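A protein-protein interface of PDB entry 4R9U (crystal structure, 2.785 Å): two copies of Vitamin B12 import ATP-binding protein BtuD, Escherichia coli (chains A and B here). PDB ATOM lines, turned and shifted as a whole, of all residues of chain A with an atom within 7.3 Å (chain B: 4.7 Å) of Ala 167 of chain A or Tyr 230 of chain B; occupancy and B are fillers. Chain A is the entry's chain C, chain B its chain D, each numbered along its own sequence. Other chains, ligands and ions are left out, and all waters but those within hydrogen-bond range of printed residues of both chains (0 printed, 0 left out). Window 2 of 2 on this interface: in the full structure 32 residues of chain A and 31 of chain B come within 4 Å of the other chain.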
ATOM      1  N   ALA A 113      -8.251 -13.445  -5.655  1.00  0.00           N
ATOM      2  CA  ALA A 113      -8.119 -14.842  -5.275  1.00  0.00           C
ATOM      3  C   ALA A 113      -6.662 -15.236  -5.124  1.00  0.00           C
ATOM      4  O   ALA A 113      -6.301 -15.970  -4.213  1.00  0.00           O
ATOM      5  CB  ALA A 113      -8.781 -15.728  -6.295  1.00  0.00           C
ATOM      6  N   LEU A 164       5.093 -21.091  -6.113  1.00  0.00           N
ATOM      7  CA  LEU A 164       3.897 -20.652  -5.419  1.00  0.00           C
ATOM      8  C   LEU A 164       3.950 -21.191  -3.996  1.00  0.00           C
ATOM      9  O   LEU A 164       4.212 -22.390  -3.837  1.00  0.00           O
ATOM     10  CB  LEU A 164       2.667 -21.188  -6.142  1.00  0.00           C
ATOM     11  CG  LEU A 164       2.255 -20.384  -7.360  1.00  0.00           C
ATOM     12  CD1 LEU A 164       0.829 -20.729  -7.721  1.00  0.00           C
ATOM     13  CD2 LEU A 164       2.397 -18.929  -7.002  1.00  0.00           C
ATOM     14  N   ASP A 165       3.701 -20.369  -2.967  1.00  0.00           N
ATOM     15  CA  ASP A 165       3.712 -20.901  -1.577  1.00  0.00           C
ATOM     16  C   ASP A 165       2.501 -21.821  -1.379  1.00  0.00           C
ATOM     17  O   ASP A 165       1.593 -21.863  -2.215  1.00  0.00           O
ATOM     18  CB  ASP A 165       3.754 -19.789  -0.492  1.00  0.00           C
ATOM     19  CG  ASP A 165       2.491 -18.924  -0.436  1.00  0.00           C
ATOM     20  OD1 ASP A 165       1.355 -19.448  -0.480  1.00  0.00           O
ATOM     21  OD2 ASP A 165       2.655 -17.679  -0.329  1.00  0.00           O
ATOM     22  N   VAL A 166       2.529 -22.593  -0.304  1.00  0.00           N
ATOM     23  CA  VAL A 166       1.477 -23.551   0.015  1.00  0.00           C
ATOM     24  C   VAL A 166       0.069 -22.979  -0.080  1.00  0.00           C
ATOM     25  O   VAL A 166      -0.814 -23.571  -0.714  1.00  0.00           O
ATOM     26  CB  VAL A 166       1.705 -24.082   1.410  1.00  0.00           C
ATOM     27  CG1 VAL A 166       0.690 -25.124   1.730  1.00  0.00           C
ATOM     28  CG2 VAL A 166       3.065 -24.672   1.445  1.00  0.00           C
ATOM     29  N   ALA A 167      -0.113 -21.811   0.525  1.00  0.00           N
ATOM     30  CA  ALA A 167      -1.395 -21.134   0.552  1.00  0.00           C
ATOM     31  C   ALA A 167      -1.824 -20.831  -0.872  1.00  0.00           C
ATOM     32  O   ALA A 167      -2.898 -21.238  -1.301  1.00  0.00           O
ATOM     33  CB  ALA A 167      -1.296 -19.861   1.365  1.00  0.00           C
ATOM     34  N   GLN A 168      -0.972 -20.129  -1.613  1.00  0.00           N
ATOM     35  CA  GLN A 168      -1.263 -19.813  -2.995  1.00  0.00           C
ATOM     36  C   GLN A 168      -1.563 -21.072  -3.816  1.00  0.00           C
ATOM     37  O   GLN A 168      -2.440 -21.062  -4.682  1.00  0.00           O
ATOM     38  CB  GLN A 168      -0.128 -19.029  -3.628  1.00  0.00           C
ATOM     39  CG  GLN A 168       0.077 -17.592  -3.116  1.00  0.00           C
ATOM     40  CD  GLN A 168      -1.179 -16.906  -2.563  1.00  0.00           C
ATOM     41  OE1 GLN A 168      -2.241 -16.842  -3.201  1.00  0.00           O
ATOM     42  NE2 GLN A 168      -1.012 -16.291  -1.398  1.00  0.00           N
ATOM     43  N   GLN A 169      -0.793 -22.139  -3.588  1.00  0.00           N
ATOM     44  CA  GLN A 169      -1.021 -23.403  -4.294  1.00  0.00           C
ATOM     45  C   GLN A 169      -2.451 -23.807  -4.067  1.00  0.00           C
ATOM     46  O   GLN A 169      -3.176 -24.069  -5.017  1.00  0.00           O
ATOM     47  CB  GLN A 169      -0.063 -24.509  -3.846  1.00  0.00           C
ATOM     48  CG  GLN A 169       1.377 -24.288  -4.301  1.00  0.00           C
ATOM     49  CD  GLN A 169       2.299 -25.411  -3.888  1.00  0.00           C
ATOM     50  OE1 GLN A 169       1.847 -26.474  -3.476  1.00  0.00           O
ATOM     51  NE2 GLN A 169       3.600 -25.174  -3.977  1.00  0.00           N
ATOM     52  N   SER A 170      -2.858 -23.812  -2.799  1.00  0.00           N
ATOM     53  CA  SER A 170      -4.233 -24.119  -2.411  1.00  0.00           C
ATOM     54  C   SER A 170      -5.269 -23.216  -3.106  1.00  0.00           C
ATOM     55  O   SER A 170      -6.306 -23.700  -3.587  1.00  0.00           O
ATOM     56  CB  SER A 170      -4.373 -23.988  -0.894  1.00  0.00           C
ATOM     57  OG  SER A 170      -5.473 -24.740  -0.422  1.00  0.00           O
ATOM     58  N   ALA A 171      -4.978 -21.915  -3.194  1.00  0.00           N
ATOM     59  CA  ALA A 171      -5.879 -20.954  -3.843  1.00  0.00           C
ATOM     60  C   ALA A 171      -6.107 -21.256  -5.345  1.00  0.00           C
ATOM     61  O   ALA A 171      -7.257 -21.374  -5.827  1.00  0.00           O
ATOM     62  CB  ALA A 171      -5.335 -19.543  -3.661  1.00  0.00           C
ATOM     63  N   LEU A 172      -5.001 -21.436  -6.059  1.00  0.00           N
ATOM     64  CA  LEU A 172      -5.062 -21.868  -7.455  1.00  0.00           C
ATOM     65  C   LEU A 172      -5.821 -23.192  -7.595  1.00  0.00           C
ATOM     66  O   LEU A 172      -6.534 -23.427  -8.587  1.00  0.00           O
ATOM     67  CB  LEU A 172      -3.657 -22.032  -8.023  1.00  0.00           C
ATOM     68  CG  LEU A 172      -3.604 -22.582  -9.448  1.00  0.00           C
ATOM     69  CD1 LEU A 172      -4.420 -21.708 -10.369  1.00  0.00           C
ATOM     70  CD2 LEU A 172      -2.163 -22.714  -9.956  1.00  0.00           C
ATOM     71  N   ASP A 173      -5.625 -24.087  -6.637  1.00  0.00           N
ATOM     72  CA  ASP A 173      -6.375 -25.326  -6.692  1.00  0.00           C
ATOM     73  C   ASP A 173      -7.868 -25.073  -6.676  1.00  0.00           C
ATOM     74  O   ASP A 173      -8.596 -25.657  -7.482  1.00  0.00           O
ATOM     75  CB  ASP A 173      -5.978 -26.263  -5.571  1.00  0.00           C
ATOM     76  CG  ASP A 173      -4.738 -27.041  -5.924  1.00  0.00           C
ATOM     77  OD1 ASP A 173      -4.655 -27.478  -7.099  1.00  0.00           O
ATOM     78  OD2 ASP A 173      -3.855 -27.193  -5.049  1.00  0.00           O
ATOM     79  N   LYS A 174      -8.328 -24.220  -5.756  1.00  0.00           N
ATOM     80  CA  LYS A 174      -9.760 -23.868  -5.709  1.00  0.00           C
ATOM     81  C   LYS A 174     -10.242 -23.288  -7.034  1.00  0.00           C
ATOM     82  O   LYS A 174     -11.315 -23.646  -7.517  1.00  0.00           O
ATOM     83  CB  LYS A 174     -10.036 -22.904  -4.557  1.00  0.00           C
ATOM     84  CG  LYS A 174      -9.644 -23.483  -3.174  1.00  0.00           C
ATOM     85  CD  LYS A 174      -9.553 -22.413  -2.083  1.00  0.00           C
ATOM     86  CE  LYS A 174      -9.163 -22.977  -0.718  1.00  0.00           C
ATOM     87  NZ  LYS A 174      -9.247 -21.906   0.318  1.00  0.00           N
ATOM     88  N   VAL B  32      12.166 -21.030   4.931  1.00  0.00           N
ATOM     89  CA  VAL B  32      10.791 -21.238   4.524  1.00  0.00           C
ATOM     90  C   VAL B  32       9.892 -20.030   4.829  1.00  0.00           C
ATOM     91  O   VAL B  32      10.155 -19.276   5.757  1.00  0.00           O
ATOM     92  CB  VAL B  32      10.217 -22.479   5.171  1.00  0.00           C
ATOM     93  CG1 VAL B  32       9.109 -22.997   4.289  1.00  0.00           C
ATOM     94  CG2 VAL B  32      11.307 -23.549   5.357  1.00  0.00           C
ATOM     95  N   GLY B  33       8.836 -19.853   4.038  1.00  0.00           N
ATOM     96  CA  GLY B  33       7.951 -18.715   4.191  1.00  0.00           C
ATOM     97  C   GLY B  33       7.220 -18.413   2.907  1.00  0.00           C
ATOM     98  O   GLY B  33       7.668 -18.794   1.818  1.00  0.00           O
ATOM     99  N   PRO B  34       6.087 -17.714   3.022  1.00  0.00           N
ATOM    100  CA  PRO B  34       5.188 -17.462   1.893  1.00  0.00           C
ATOM    101  C   PRO B  34       5.832 -16.578   0.836  1.00  0.00           C
ATOM    102  O   PRO B  34       6.907 -16.047   1.073  1.00  0.00           O
ATOM    103  CB  PRO B  34       4.016 -16.731   2.548  1.00  0.00           C
ATOM    104  CG  PRO B  34       4.596 -16.110   3.788  1.00  0.00           C
ATOM    105  CD  PRO B  34       5.626 -17.070   4.265  1.00  0.00           C
ATOM    106  N   HIS B 191       9.870 -24.447  -0.764  1.00  0.00           N
ATOM    107  CA  HIS B 191       8.449 -24.312  -0.535  1.00  0.00           C
ATOM    108  C   HIS B 191       7.813 -25.665  -0.268  1.00  0.00           C
ATOM    109  O   HIS B 191       6.614 -25.723  -0.046  1.00  0.00           O
ATOM    110  CB  HIS B 191       7.742 -23.645  -1.698  1.00  0.00           C
ATOM    111  CG  HIS B 191       7.671 -22.162  -1.572  1.00  0.00           C
ATOM    112  ND1 HIS B 191       8.271 -21.309  -2.480  1.00  0.00           N
ATOM    113  CD2 HIS B 191       7.109 -21.376  -0.623  1.00  0.00           C
ATOM    114  CE1 HIS B 191       8.062 -20.060  -2.105  1.00  0.00           C
ATOM    115  NE2 HIS B 191       7.365 -20.074  -0.980  1.00  0.00           N
ATOM    116  N   LEU B 193       7.351 -28.094   2.310  1.00  0.00           N
ATOM    117  CA  LEU B 193       7.520 -28.315   3.747  1.00  0.00           C
ATOM    118  C   LEU B 193       7.999 -29.722   4.083  1.00  0.00           C
ATOM    119  O   LEU B 193       8.921 -29.872   4.877  1.00  0.00           O
ATOM    120  CB  LEU B 193       6.241 -28.056   4.522  1.00  0.00           C
ATOM    121  CG  LEU B 193       5.754 -26.630   4.711  1.00  0.00           C
ATOM    122  CD1 LEU B 193       6.732 -25.533   4.293  1.00  0.00           C
ATOM    123  CD2 LEU B 193       4.595 -26.667   3.780  1.00  0.00           C
ATOM    124  N   LEU B 226       3.036 -22.732  11.383  1.00  0.00           N
ATOM    125  CA  LEU B 226       2.668 -22.764   9.973  1.00  0.00           C
ATOM    126  C   LEU B 226       1.341 -22.074   9.779  1.00  0.00           C
ATOM    127  O   LEU B 226       1.110 -21.433   8.745  1.00  0.00           O
ATOM    128  CB  LEU B 226       2.599 -24.191   9.445  1.00  0.00           C
ATOM    129  CG  LEU B 226       3.908 -24.964   9.609  1.00  0.00           C
ATOM    130  CD1 LEU B 226       3.761 -26.416   9.152  1.00  0.00           C
ATOM    131  CD2 LEU B 226       5.032 -24.262   8.880  1.00  0.00           C
ATOM    132  N   ALA B 227       0.491 -22.156  10.795  1.00  0.00           N
ATOM    133  CA  ALA B 227      -0.795 -21.477  10.744  1.00  0.00           C
ATOM    134  C   ALA B 227      -0.592 -19.966  10.771  1.00  0.00           C
ATOM    135  O   ALA B 227      -1.320 -19.231  10.114  1.00  0.00           O
ATOM    136  CB  ALA B 227      -1.700 -21.909  11.895  1.00  0.00           C
ATOM    137  N   GLN B 228       0.372 -19.479  11.533  1.00  0.00           N
ATOM    138  CA  GLN B 228       0.599 -18.043  11.459  1.00  0.00           C
ATOM    139  C   GLN B 228       1.183 -17.610  10.128  1.00  0.00           C
ATOM    140  O   GLN B 228       0.732 -16.625   9.537  1.00  0.00           O
ATOM    141  CB  GLN B 228       1.479 -17.572  12.595  1.00  0.00           C
ATOM    142  CG  GLN B 228       0.696 -17.374  13.850  1.00  0.00           C
ATOM    143  CD  GLN B 228       1.457 -16.548  14.834  1.00  0.00           C
ATOM    144  OE1 GLN B 228       2.550 -16.068  14.526  1.00  0.00           O
ATOM    145  NE2 GLN B 228       0.898 -16.368  16.030  1.00  0.00           N
ATOM    146  N   ALA B 229       2.167 -18.358   9.647  1.00  0.00           N
ATOM    147  CA  ALA B 229       2.878 -17.969   8.431  1.00  0.00           C
ATOM    148  C   ALA B 229       2.019 -18.045   7.173  1.00  0.00           C
ATOM    149  O   ALA B 229       1.912 -17.072   6.415  1.00  0.00           O
ATOM    150  CB  ALA B 229       4.094 -18.825   8.259  1.00  0.00           C
ATOM    151  N   TYR B 230       1.410 -19.193   6.929  1.00  0.00           N
ATOM    152  CA  TYR B 230       0.644 -19.376   5.713  1.00  0.00           C
ATOM    153  C   TYR B 230      -0.836 -19.038   5.861  1.00  0.00           C
ATOM    154  O   TYR B 230      -1.514 -18.742   4.879  1.00  0.00           O
ATOM    155  CB  TYR B 230       0.838 -20.805   5.224  1.00  0.00           C
ATOM    156  CG  TYR B 230       2.276 -21.056   4.826  1.00  0.00           C
ATOM    157  CD1 TYR B 230       3.182 -21.555   5.737  1.00  0.00           C
ATOM    158  CD2 TYR B 230       2.749 -20.698   3.573  1.00  0.00           C
ATOM    159  CE1 TYR B 230       4.500 -21.767   5.400  1.00  0.00           C
ATOM    160  CE2 TYR B 230       4.073 -20.910   3.226  1.00  0.00           C
ATOM    161  CZ  TYR B 230       4.941 -21.440   4.145  1.00  0.00           C
ATOM    162  OH  TYR B 230       6.263 -21.640   3.799  1.00  0.00           O
ATOM    163  N   GLY B 231      -1.344 -19.146   7.088  1.00  0.00           N
ATOM    164  CA  GLY B 231      -2.745 -18.887   7.361  1.00  0.00           C
ATOM    165  C   GLY B 231      -3.626 -20.093   7.050  1.00  0.00           C
ATOM    166  O   GLY B 231      -4.618 -19.979   6.329  1.00  0.00           O
ATOM    167  N   MET B 232      -3.286 -21.252   7.605  1.00  0.00           N
ATOM    168  CA  MET B 232      -4.106 -22.449   7.394  1.00  0.00           C
ATOM    169  C   MET B 232      -3.711 -23.597   8.299  1.00  0.00           C
ATOM    170  O   MET B 232      -2.536 -23.779   8.620  1.00  0.00           O
ATOM    171  CB  MET B 232      -4.055 -22.923   5.933  1.00  0.00           C
ATOM    172  CG  MET B 232      -2.687 -23.017   5.330  1.00  0.00           C
ATOM    173  SD  MET B 232      -2.808 -23.091   3.528  1.00  0.00           S
ATOM    174  CE  MET B 232      -3.487 -24.731   3.239  1.00  0.00           C
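OD1 of Asp 165 of chain A lies within hydrogen-bond range of N of Gln 168 of chain A.
O of Gly 33 of chain B is in hydrogen-bond range of NE2 of His 191 of chain B (3.1 Å).
OH of Tyr 230 of chain B lies within hydrogen-bond range of N of Gly 33 of chain B (3.1 Å).
N of Ala 167 of chain A sits at hydrogen-bond distance from OD1 of Asp 165 of chain A, at 3.0 Å.
Pro 34 of chain B touches Asp 165 of chain A (CB to OD2, 3.3 Å).
Asp 165 of chain A touches His 191 of chain B (CA to CD2, 3.6 Å).
Tyr 230 of chain B touches Asp 165 of chain A (CE2 to CB, 3.9 Å).
CG2 of Val 166 of chain A touches O of His 191 of chain B, at 3.99 Å.
CG2 of Val 166 of chain A touches CD2 of Leu 193 of chain B, at 3.4 Å.
CB of Ala 167 of chain A touches O of Tyr 230 of chain B, at 3.7 Å.
Ala 167 of chain A touches Met 232 of chain B (CA to SD, 3.8 Å).
Of chain A, only Asp 165 (3.9 Å) and Ala 167 (3.7 Å) come within 4 Å of Tyr 230 of chain B.
No residue of chain A comes within 4 Å of Ala 229 of chain B.
Of the printed residues of chain B, Val 166 of chain A touches His 191 (3.99 Å) and Leu 193 (3.4 Å).
Printed residues of chain A within 4 Å of His 191 of chain B: Asp 165 and Val 166.
Printed residues of chain A within 4 Å of Met 232 of chain B: Ala 167 (3.8 Å).
Of the printed residues of chain A, Leu 193 of chain B touches Val 166.
Leu 164 of chain A touches none of the printed residues of chain B.
Gly 33 of chain B touches none of the printed residues of chain A.
The nearest residue of chain A that does not touch Tyr 230 of chain B is Val 166 of chain A (4.1 Å).
The nearest printed residue of chain B that does not touch Val 166 of chain A is Tyr 230 of chain B (4.1 Å).
Hydrophobic or aromatic side chains of chain A within 4 Å of the printed part of chain B: Val 166 and Ala 167.
Printed residues of chain B that touch a printed residue of chain A: Pro 34, His 191, Leu 193, Tyr 230 and Met 232.
Hydrophobic or aromatic side chains of chain B that line the printed part of chain A: Pro 34, His 191, Leu 193, Tyr 230 and Met 232.
Among the printed residues, 7 pairs touch across the chains.
Among the printed residues, no Asp or Glu carboxylate lies within 4 Å of a Lys or Arg side-chain nitrogen of the other chain.
No position is printed for both chains.
Of the 7 pairs that touch across the chains among the printed residues, none has its exchanged pair printed and touching as well.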
